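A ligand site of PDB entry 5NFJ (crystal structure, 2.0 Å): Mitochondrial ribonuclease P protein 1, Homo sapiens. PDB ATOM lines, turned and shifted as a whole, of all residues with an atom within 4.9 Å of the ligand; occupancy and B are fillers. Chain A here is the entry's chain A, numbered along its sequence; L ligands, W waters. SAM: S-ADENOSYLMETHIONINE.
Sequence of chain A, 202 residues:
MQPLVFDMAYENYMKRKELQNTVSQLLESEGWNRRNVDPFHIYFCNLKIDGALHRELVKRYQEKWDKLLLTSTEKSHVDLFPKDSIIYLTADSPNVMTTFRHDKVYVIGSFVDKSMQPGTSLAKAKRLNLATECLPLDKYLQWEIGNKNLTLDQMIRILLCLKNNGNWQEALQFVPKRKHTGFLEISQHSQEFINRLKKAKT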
ATOM      1  N   TYR A  10      -0.173 -10.764  -4.907  1.00  0.00           N
ATOM      2  CA  TYR A  10      -1.425 -11.539  -5.007  1.00  0.00           C
ATOM      3  C   TYR A  10      -2.102 -11.487  -6.289  1.00  0.00           C
ATOM      4  O   TYR A  10      -3.217 -12.016  -6.476  1.00  0.00           O
ATOM      5  CB  TYR A  10      -2.406 -11.106  -3.933  1.00  0.00           C
ATOM      6  CG  TYR A  10      -1.913 -11.253  -2.558  1.00  0.00           C
ATOM      7  CD1 TYR A  10      -1.102 -10.273  -1.979  1.00  0.00           C
ATOM      8  CD2 TYR A  10      -2.279 -12.336  -1.792  1.00  0.00           C
ATOM      9  CE1 TYR A  10      -0.668 -10.383  -0.697  1.00  0.00           C
ATOM     10  CE2 TYR A  10      -1.842 -12.452  -0.477  1.00  0.00           C
ATOM     11  CZ  TYR A  10      -0.995 -11.514   0.069  1.00  0.00           C
ATOM     12  OH  TYR A  10      -0.579 -11.672   1.408  1.00  0.00           O
ATOM     13  N   TYR A  88       3.105  -9.103   9.880  1.00  0.00           N
ATOM     14  CA  TYR A  88       2.152  -9.287   8.787  1.00  0.00           C
ATOM     15  C   TYR A  88       0.752  -9.361   9.395  1.00  0.00           C
ATOM     16  O   TYR A  88       0.495 -10.171  10.307  1.00  0.00           O
ATOM     17  CB  TYR A  88       2.488 -10.491   7.950  1.00  0.00           C
ATOM     18  CG  TYR A  88       2.172 -10.379   6.474  1.00  0.00           C
ATOM     19  CD1 TYR A  88       0.870 -10.130   6.017  1.00  0.00           C
ATOM     20  CD2 TYR A  88       3.148 -10.533   5.520  1.00  0.00           C
ATOM     21  CE1 TYR A  88       0.613  -9.996   4.646  1.00  0.00           C
ATOM     22  CE2 TYR A  88       2.875 -10.413   4.158  1.00  0.00           C
ATOM     23  CZ  TYR A  88       1.570 -10.124   3.725  1.00  0.00           C
ATOM     24  OH  TYR A  88       1.313 -10.026   2.343  1.00  0.00           O
ATOM     25  N   LEU A  89      -0.137  -8.433   8.971  1.00  0.00           N
ATOM     26  CA  LEU A  89      -1.501  -8.381   9.466  1.00  0.00           C
ATOM     27  C   LEU A  89      -2.333  -9.357   8.670  1.00  0.00           C
ATOM     28  O   LEU A  89      -2.312  -9.313   7.429  1.00  0.00           O
ATOM     29  CB  LEU A  89      -2.099  -6.939   9.362  1.00  0.00           C
ATOM     30  CG  LEU A  89      -1.470  -5.928  10.366  1.00  0.00           C
ATOM     31  CD1 LEU A  89      -1.851  -4.432  10.242  1.00  0.00           C
ATOM     32  CD2 LEU A  89      -1.675  -6.378  11.778  1.00  0.00           C
ATOM     33  N   THR A  90      -3.122 -10.205   9.365  1.00  0.00           N
ATOM     34  CA  THR A  90      -4.075 -11.112   8.672  1.00  0.00           C
ATOM     35  C   THR A  90      -5.168 -11.595   9.656  1.00  0.00           C
ATOM     36  O   THR A  90      -4.900 -11.831  10.825  1.00  0.00           O
ATOM     37  CB  THR A  90      -3.365 -12.294   7.944  1.00  0.00           C
ATOM     38  OG1 THR A  90      -4.326 -13.264   7.404  1.00  0.00           O
ATOM     39  CG2 THR A  90      -2.410 -12.975   8.884  1.00  0.00           C
ATOM     40  N   ALA A  91      -6.437 -11.595   9.213  1.00  0.00           N
ATOM     41  CA  ALA A  91      -7.536 -11.955  10.098  1.00  0.00           C
ATOM     42  C   ALA A  91      -7.377 -13.464  10.485  1.00  0.00           C
ATOM     43  O   ALA A  91      -7.752 -13.831  11.568  1.00  0.00           O
ATOM     44  CB  ALA A  91      -8.906 -11.726   9.472  1.00  0.00           C
ATOM     45  N   ASP A  92      -6.806 -14.267   9.596  1.00  0.00           N
ATOM     46  CA  ASP A  92      -6.491 -15.668   9.895  1.00  0.00           C
ATOM     47  C   ASP A  92      -5.385 -15.879  10.946  1.00  0.00           C
ATOM     48  O   ASP A  92      -5.238 -17.000  11.387  1.00  0.00           O
ATOM     49  CB  ASP A  92      -6.125 -16.429   8.628  1.00  0.00           C
ATOM     50  CG  ASP A  92      -7.241 -16.470   7.605  1.00  0.00           C
ATOM     51  OD1 ASP A  92      -8.411 -16.485   8.037  1.00  0.00           O
ATOM     52  OD2 ASP A  92      -6.971 -16.501   6.360  1.00  0.00           O
ATOM     53  N   VAL A 107       2.469  -4.978   7.693  1.00  0.00           N
ATOM     54  CA  VAL A 107       2.309  -5.358   6.289  1.00  0.00           C
ATOM     55  C   VAL A 107       0.851  -5.730   6.067  1.00  0.00           C
ATOM     56  O   VAL A 107       0.288  -6.510   6.876  1.00  0.00           O
ATOM     57  CB  VAL A 107       3.226  -6.549   5.846  1.00  0.00           C
ATOM     58  CG1 VAL A 107       3.082  -6.846   4.352  1.00  0.00           C
ATOM     59  CG2 VAL A 107       4.682  -6.232   6.115  1.00  0.00           C
ATOM     60  N   ILE A 108       0.268  -5.272   4.962  1.00  0.00           N
ATOM     61  CA  ILE A 108      -1.131  -5.549   4.626  1.00  0.00           C
ATOM     62  C   ILE A 108      -1.079  -6.200   3.262  1.00  0.00           C
ATOM     63  O   ILE A 108      -0.419  -5.686   2.305  1.00  0.00           O
ATOM     64  CB  ILE A 108      -1.976  -4.189   4.558  1.00  0.00           C
ATOM     65  CG1 ILE A 108      -2.133  -3.547   5.901  1.00  0.00           C
ATOM     66  CG2 ILE A 108      -3.333  -4.371   3.923  1.00  0.00           C
ATOM     67  CD1 ILE A 108      -2.365  -2.041   5.831  1.00  0.00           C
ATOM     68  N   GLY A 109      -1.833  -7.282   3.075  1.00  0.00           N
ATOM     69  CA  GLY A 109      -1.909  -7.908   1.749  1.00  0.00           C
ATOM     70  C   GLY A 109      -2.838  -7.194   0.760  1.00  0.00           C
ATOM     71  O   GLY A 109      -4.019  -6.952   1.096  1.00  0.00           O
ATOM     72  N   PHE A 111      -5.052  -7.582  -1.665  1.00  0.00           N
ATOM     73  CA  PHE A 111      -5.792  -8.729  -2.124  1.00  0.00           C
ATOM     74  C   PHE A 111      -7.291  -8.561  -1.839  1.00  0.00           C
ATOM     75  O   PHE A 111      -7.664  -8.306  -0.708  1.00  0.00           O
ATOM     76  CB  PHE A 111      -5.247  -9.954  -1.357  1.00  0.00           C
ATOM     77  CG  PHE A 111      -5.734 -11.321  -1.880  1.00  0.00           C
ATOM     78  CD1 PHE A 111      -6.101 -11.534  -3.178  1.00  0.00           C
ATOM     79  CD2 PHE A 111      -5.699 -12.417  -1.018  1.00  0.00           C
ATOM     80  CE1 PHE A 111      -6.449 -12.808  -3.629  1.00  0.00           C
ATOM     81  CE2 PHE A 111      -6.065 -13.701  -1.448  1.00  0.00           C
ATOM     82  CZ  PHE A 111      -6.438 -13.879  -2.743  1.00  0.00           C
ATOM     83  N   VAL A 112      -8.073  -8.605  -2.890  1.00  0.00           N
ATOM     84  CA  VAL A 112      -9.530  -8.682  -2.755  1.00  0.00           C
ATOM     85  C   VAL A 112      -9.935 -10.099  -3.267  1.00  0.00           C
ATOM     86  O   VAL A 112      -9.773 -10.374  -4.463  1.00  0.00           O
ATOM     87  CB  VAL A 112     -10.206  -7.580  -3.622  1.00  0.00           C
ATOM     88  CG1 VAL A 112     -11.695  -7.804  -3.722  1.00  0.00           C
ATOM     89  CG2 VAL A 112      -9.895  -6.158  -3.103  1.00  0.00           C
ATOM     90  N   ASP A 113     -10.468 -10.903  -2.360  1.00  0.00           N
ATOM     91  CA  ASP A 113     -10.950 -12.294  -2.632  1.00  0.00           C
ATOM     92  C   ASP A 113     -12.431 -12.603  -2.244  1.00  0.00           C
ATOM     93  O   ASP A 113     -12.944 -13.703  -2.589  1.00  0.00           O
ATOM     94  CB  ASP A 113     -10.088 -13.332  -1.848  1.00  0.00           C
ATOM     95  CG  ASP A 113     -10.253 -13.213  -0.364  1.00  0.00           C
ATOM     96  OD1 ASP A 113     -10.567 -12.088   0.093  1.00  0.00           O
ATOM     97  OD2 ASP A 113     -10.066 -14.233   0.365  1.00  0.00           O
ATOM     98  N   GLN A 117     -10.825 -17.126  -0.274  1.00  0.00           N
ATOM     99  CA  GLN A 117      -9.422 -17.647  -0.391  1.00  0.00           C
ATOM    100  C   GLN A 117      -8.706 -17.473   0.893  1.00  0.00           C
ATOM    101  O   GLN A 117      -7.674 -16.867   0.932  1.00  0.00           O
ATOM    102  CB  GLN A 117      -8.674 -17.021  -1.536  1.00  0.00           C
ATOM    103  CG  GLN A 117      -9.297 -17.310  -2.885  1.00  0.00           C
ATOM    104  CD  GLN A 117      -8.575 -16.663  -4.026  1.00  0.00           C
ATOM    105  OE1 GLN A 117      -7.529 -17.113  -4.505  1.00  0.00           O
ATOM    106  NE2 GLN A 117      -9.208 -15.627  -4.560  1.00  0.00           N
ATOM    107  N   PRO A 118      -9.250 -18.080   1.980  1.00  0.00           N
ATOM    108  CA  PRO A 118      -8.630 -17.968   3.261  1.00  0.00           C
ATOM    109  C   PRO A 118      -7.287 -18.689   3.326  1.00  0.00           C
ATOM    110  O   PRO A 118      -6.891 -19.458   2.386  1.00  0.00           O
ATOM    111  CB  PRO A 118      -9.659 -18.618   4.197  1.00  0.00           C
ATOM    112  CG  PRO A 118     -10.253 -19.681   3.368  1.00  0.00           C
ATOM    113  CD  PRO A 118     -10.211 -19.193   1.945  1.00  0.00           C
ATOM    114  N   GLY A 119      -6.576 -18.271   4.362  1.00  0.00           N
ATOM    115  CA  GLY A 119      -5.177 -18.570   4.614  1.00  0.00           C
ATOM    116  C   GLY A 119      -4.098 -18.053   3.708  1.00  0.00           C
ATOM    117  O   GLY A 119      -2.912 -18.404   3.897  1.00  0.00           O
ATOM    118  N   THR A 120      -4.458 -17.271   2.685  1.00  0.00           N
ATOM    119  CA  THR A 120      -3.505 -16.997   1.641  1.00  0.00           C
ATOM    120  C   THR A 120      -2.293 -16.183   2.165  1.00  0.00           C
ATOM    121  O   THR A 120      -1.091 -16.483   1.852  1.00  0.00           O
ATOM    122  CB  THR A 120      -4.156 -16.373   0.426  1.00  0.00           C
ATOM    123  OG1 THR A 120      -5.273 -17.182  -0.002  1.00  0.00           O
ATOM    124  CG2 THR A 120      -3.119 -16.263  -0.769  1.00  0.00           C
ATOM    125  N   SER A 121      -2.600 -15.215   3.020  1.00  0.00           N
ATOM    126  CA  SER A 121      -1.605 -14.263   3.437  1.00  0.00           C
ATOM    127  C   SER A 121      -0.896 -14.822   4.654  1.00  0.00           C
ATOM    128  O   SER A 121       0.300 -14.686   4.736  1.00  0.00           O
ATOM    129  CB  SER A 121      -2.198 -12.870   3.674  1.00  0.00           C
ATOM    130  OG  SER A 121      -3.086 -12.792   4.740  1.00  0.00           O
ATOM    131  N   GLU A 133      -0.328 -10.963  13.194  1.00  0.00           N
ATOM    132  CA  GLU A 133      -1.366 -10.548  14.138  1.00  0.00           C
ATOM    133  C   GLU A 133      -2.710 -10.310  13.395  1.00  0.00           C
ATOM    134  O   GLU A 133      -2.752  -9.997  12.178  1.00  0.00           O
ATOM    135  CB  GLU A 133      -1.055  -9.286  14.978  1.00  0.00           C
ATOM    136  CG  GLU A 133       0.109  -9.318  15.951  1.00  0.00           C
ATOM    137  CD  GLU A 133       0.290  -8.020  16.727  1.00  0.00           C
ATOM    138  OE1 GLU A 133       0.357  -6.910  16.165  1.00  0.00           O
ATOM    139  OE2 GLU A 133       0.373  -8.076  17.943  1.00  0.00           O
ATOM    140  N   CYS A 134      -3.801 -10.483  14.149  1.00  0.00           N
ATOM    141  CA  CYS A 134      -5.129 -10.162  13.671  1.00  0.00           C
ATOM    142  C   CYS A 134      -5.704  -9.022  14.541  1.00  0.00           C
ATOM    143  O   CYS A 134      -5.252  -8.770  15.665  1.00  0.00           O
ATOM    144  CB  CYS A 134      -6.041 -11.399  13.654  1.00  0.00           C
ATOM    145  SG  CYS A 134      -6.543 -11.970  15.292  1.00  0.00           S
ATOM    146  N   LEU A 135      -6.701  -8.319  13.993  1.00  0.00           N
ATOM    147  CA  LEU A 135      -7.292  -7.225  14.722  1.00  0.00           C
ATOM    148  C   LEU A 135      -8.287  -7.875  15.719  1.00  0.00           C
ATOM    149  O   LEU A 135      -8.906  -8.875  15.342  1.00  0.00           O
ATOM    150  CB  LEU A 135      -8.038  -6.228  13.803  1.00  0.00           C
ATOM    151  CG  LEU A 135      -7.225  -5.284  12.888  1.00  0.00           C
ATOM    152  CD1 LEU A 135      -8.177  -4.523  11.970  1.00  0.00           C
ATOM    153  CD2 LEU A 135      -6.393  -4.323  13.719  1.00  0.00           C
ATOM    154  N   LEU A 137     -11.365  -7.881  16.541  1.00  0.00           N
ATOM    155  CA  LEU A 137     -12.742  -7.542  16.160  1.00  0.00           C
ATOM    156  C   LEU A 137     -13.783  -8.223  17.080  1.00  0.00           C
ATOM    157  O   LEU A 137     -14.787  -7.611  17.421  1.00  0.00           O
ATOM    158  CB  LEU A 137     -13.009  -7.898  14.679  1.00  0.00           C
ATOM    159  CG  LEU A 137     -12.076  -7.232  13.648  1.00  0.00           C
ATOM    160  CD1 LEU A 137     -12.512  -7.507  12.239  1.00  0.00           C
ATOM    161  CD2 LEU A 137     -11.948  -5.738  13.914  1.00  0.00           C
ATOM    162  N   LYS A 148     -15.008 -10.598   8.826  1.00  0.00           N
ATOM    163  CA  LYS A 148     -13.823 -10.080   9.501  1.00  0.00           C
ATOM    164  C   LYS A 148     -12.641  -9.643   8.559  1.00  0.00           C
ATOM    165  O   LYS A 148     -11.701  -9.094   9.040  1.00  0.00           O
ATOM    166  CB  LYS A 148     -13.334 -11.078  10.566  1.00  0.00           C
ATOM    167  CG  LYS A 148     -14.067 -10.893  11.900  1.00  0.00           C
ATOM    168  CD  LYS A 148     -13.683 -11.914  12.977  1.00  0.00           C
ATOM    169  CE  LYS A 148     -14.171 -13.317  12.639  1.00  0.00           C
ATOM    170  NZ  LYS A 148     -14.191 -14.210  13.842  1.00  0.00           N
ATOM    171  N   ASN A 149     -12.705  -9.978   7.284  1.00  0.00           N
ATOM    172  CA  ASN A 149     -11.728  -9.620   6.274  1.00  0.00           C
ATOM    173  C   ASN A 149     -12.051  -8.216   5.669  1.00  0.00           C
ATOM    174  O   ASN A 149     -12.814  -8.078   4.734  1.00  0.00           O
ATOM    175  CB  ASN A 149     -11.705 -10.664   5.165  1.00  0.00           C
ATOM    176  CG  ASN A 149     -11.091 -11.981   5.628  1.00  0.00           C
ATOM    177  OD1 ASN A 149      -9.903 -12.049   5.967  1.00  0.00           O
ATOM    178  ND2 ASN A 149     -11.893 -13.001   5.699  1.00  0.00           N
ATOM    179  N   LEU A 150     -11.435  -7.221   6.266  1.00  0.00           N
ATOM    180  CA  LEU A 150     -11.643  -5.802   5.941  1.00  0.00           C
ATOM    181  C   LEU A 150     -10.944  -5.371   4.663  1.00  0.00           C
ATOM    182  O   LEU A 150     -10.086  -6.091   4.117  1.00  0.00           O
ATOM    183  CB  LEU A 150     -11.161  -5.016   7.107  1.00  0.00           C
ATOM    184  CG  LEU A 150     -11.783  -5.387   8.446  1.00  0.00           C
ATOM    185  CD1 LEU A 150     -11.323  -4.407   9.511  1.00  0.00           C
ATOM    186  CD2 LEU A 150     -13.329  -5.400   8.412  1.00  0.00           C
ATOM    187  N   LEU A 152      -8.696  -2.608   2.264  1.00  0.00           N
ATOM    188  CA  LEU A 152      -7.354  -1.977   2.472  1.00  0.00           C
ATOM    189  C   LEU A 152      -7.496  -0.561   3.063  1.00  0.00           C
ATOM    190  O   LEU A 152      -6.757  -0.200   3.933  1.00  0.00           O
ATOM    191  CB  LEU A 152      -6.622  -1.879   1.128  1.00  0.00           C
ATOM    192  CG  LEU A 152      -6.496  -3.148   0.225  1.00  0.00           C
ATOM    193  CD1 LEU A 152      -5.506  -2.938  -0.897  1.00  0.00           C
ATOM    194  CD2 LEU A 152      -5.996  -4.306   1.075  1.00  0.00           C
ATOM    195  N   MET A 155      -8.380  -0.827   6.768  1.00  0.00           N
ATOM    196  CA  MET A 155      -7.164  -1.089   7.527  1.00  0.00           C
ATOM    197  C   MET A 155      -6.342   0.193   7.744  1.00  0.00           C
ATOM    198  O   MET A 155      -5.933   0.497   8.881  1.00  0.00           O
ATOM    199  CB  MET A 155      -6.313  -2.153   6.789  1.00  0.00           C
ATOM    200  CG  MET A 155      -6.903  -3.593   6.657  1.00  0.00           C
ATOM    201  SD  MET A 155      -7.278  -4.341   8.257  1.00  0.00           S
ATOM    202  CE  MET A 155      -5.695  -4.324   9.039  1.00  0.00           C
HETATM  203  N   SAM L   1      -8.173 -14.118   2.006  1.00  0.00           N
HETATM  204  CA  SAM L   1      -7.381 -12.900   2.183  1.00  0.00           C
HETATM  205  C   SAM L   1      -6.135 -13.247   3.005  1.00  0.00           C
HETATM  206  O   SAM L   1      -5.637 -14.419   2.914  1.00  0.00           O
HETATM  207  OXT SAM L   1      -5.635 -12.360   3.759  1.00  0.00           O
HETATM  208  CB  SAM L   1      -8.229 -11.761   2.816  1.00  0.00           C
HETATM  209  CG  SAM L   1      -7.749 -10.378   2.274  1.00  0.00           C
HETATM  210  SD  SAM L   1      -8.379  -8.956   3.038  1.00  0.00           S
HETATM  211  CE  SAM L   1      -9.747  -8.709   2.089  1.00  0.00           C
HETATM  212  C5' SAM L   1      -7.231  -7.693   2.784  1.00  0.00           C
HETATM  213  C4' SAM L   1      -5.974  -7.566   3.647  1.00  0.00           C
HETATM  214  O4' SAM L   1      -6.170  -6.696   4.761  1.00  0.00           O
HETATM  215  C3' SAM L   1      -5.382  -8.862   4.273  1.00  0.00           C
HETATM  216  O3' SAM L   1      -4.375  -9.398   3.426  1.00  0.00           O
HETATM  217  C2' SAM L   1      -4.794  -8.424   5.539  1.00  0.00           C
HETATM  218  O2' SAM L   1      -3.468  -7.952   5.330  1.00  0.00           O
HETATM  219  C1' SAM L   1      -5.635  -7.221   5.973  1.00  0.00           C
HETATM  220  N9  SAM L   1      -6.751  -7.539   6.924  1.00  0.00           N
HETATM  221  C8  SAM L   1      -8.054  -7.534   6.593  1.00  0.00           C
HETATM  222  N7  SAM L   1      -8.800  -7.769   7.680  1.00  0.00           N
HETATM  223  C5  SAM L   1      -7.957  -7.915   8.720  1.00  0.00           C
HETATM  224  C6  SAM L   1      -8.103  -8.299  10.133  1.00  0.00           C
HETATM  225  N6  SAM L   1      -9.348  -8.463  10.653  1.00  0.00           N
HETATM  226  N1  SAM L   1      -6.986  -8.394  10.880  1.00  0.00           N
HETATM  227  C2  SAM L   1      -5.757  -8.208  10.335  1.00  0.00           C
HETATM  228  N3  SAM L   1      -5.579  -7.955   9.029  1.00  0.00           N
HETATM  229  C4  SAM L   1      -6.612  -7.778   8.201  1.00  0.00           C
HETATM  230  O   HOH W   1      -4.617 -15.203   5.631  1.00  0.00           O
HETATM  231  O   HOH W   2      -9.712 -10.011  13.231  1.00  0.00           O
HETATM  232  O   HOH W   3      -7.079 -11.043   6.350  1.00  0.00           O
HETATM  233  O   HOH W   4      -8.247 -14.290   4.597  1.00  0.00           O
HETATM  234  O   HOH W   5     -12.306  -8.920  -0.129  1.00  0.00           O
HETATM  235  O   HOH W   6      -9.302  -5.956   0.285  1.00  0.00           O
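A nitrogen (N9) of the ligand lies close to the side-chain sulfur (SD) of Met 155, 3.5 Å away.
CB of Ala 91 touches N6 of the ligand, 3.5 Å away.
Ile 108 touches the ligand.
O of Phe 111 touches CE of the ligand (3.5 Å).
O of Glu 133 touches C2 of the ligand, at 3.95 Å.
CA of Cys 134 touches N1 of the ligand, at 3.8 Å.
Leu 137 touches the ligand (CD1 to N6, 3.7 Å).
Asn 149 touches the ligand (OD1 to CB, 3.6 Å).
Leu 152 touches the ligand.
Hydrophobic or aromatic side chains within 4 Å of the ligand: Leu 89, Ala 91, Ile 108, Phe 111, Leu 135, Leu 137, Leu 150, Leu 152 and Met 155.
19 residues have an atom within 4 Å of the ligand: Leu 89, Thr 90, Ala 91, Ile 108, Gly 109, Phe 111, Asp 113, Gln 117, Thr 120, Ser 121, Glu 133, Cys 134, Leu 135, Leu 137, Lys 148, Asn 149, Leu 150, Leu 152 and Met 155.
The nearest printed residue that does not touch the ligand is Gly 119 (4.03 Å).
The side-chain carboxylate (OD2) of Asp 113 is in salt-bridge range of a nitrogen (N) of the ligand, at 2.5 Å.
The backbone carbonyl oxygen (O) of Leu 89 is in hydrogen-bond range of an oxygen (O2') of the ligand, 2.8 Å away.
The backbone NH (N) of Ser 121 sits at hydrogen-bond distance from an oxygen (O) of the ligand, 3.1 Å away.
An oxygen (OXT) of the ligand lies within hydrogen-bond range of the side-chain hydroxyl of Ser 121, 2.8 Å away.
O2' of the ligand sits at hydrogen-bond distance from N of Gly 109.
O of Gly 109 sits close to O3' of the ligand (3.4 Å).
The backbone carbonyl oxygen (O) of Lys 148 lies within hydrogen-bond range of a nitrogen (N6) of the ligand (2.9 Å).
O of Gln 117 is in hydrogen-bond range of N of the ligand (3.0 Å).
A nitrogen (N7) of the ligand lies within hydrogen-bond range of the backbone NH of Leu 150.
An oxygen (O) of the ligand is in hydrogen-bond range of the backbone NH (N) of Thr 120 (3.1 Å).
A nitrogen (N1) of the ligand sits at hydrogen-bond distance from the backbone NH of Leu 135 (3.1 Å).
N of Thr 90 lies within hydrogen-bond range of N3 of the ligand (3.3 Å).
Water W4 lies within hydrogen-bond range of N of the ligand, OD2 of Asp 92 and OD1 of Asn 149.
Water W1 lies within hydrogen-bond range of OG1 of Thr 90 (2.6 Å), OD2 of Asp 92 (2.8 Å), OG of Ser 121 (3.0 Å) and O of the ligand (3.0 Å).
Water W2 bridges the backbone carbonyl oxygen (O) of Leu 135 (2.5 Å) and a nitrogen (N6) of the ligand (3.0 Å).
Water W3 lies within hydrogen-bond range of N of Ala 91 (3.0 Å), OD1 of Asn 149 (3.0 Å) and OXT of the ligand (3.2 Å).
The backbone NH of Gln 117 lies within hydrogen-bond range of the side-chain carboxylate of Asp 113.
N of Leu 89 sits at hydrogen-bond distance from O of Val 107, at 2.9 Å.
OG1 of Thr 90 lies within hydrogen-bond range of OG of Ser 121 (3.0 Å).
The side-chain hydroxyl (OG1) of Thr 120 lies within hydrogen-bond range of the backbone carbonyl oxygen (O) of Gln 117.
The backbone NH (N) of Thr 90 lies within hydrogen-bond range of the backbone carbonyl oxygen (O) of Glu 133 (2.8 Å).
The side-chain hydroxyl (OG1) of Thr 90 lies close to the backbone NH (N) of Asp 92, at 3.5 Å.
N of Glu 133 lies within hydrogen-bond range of O of Tyr 88, 3.1 Å away.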
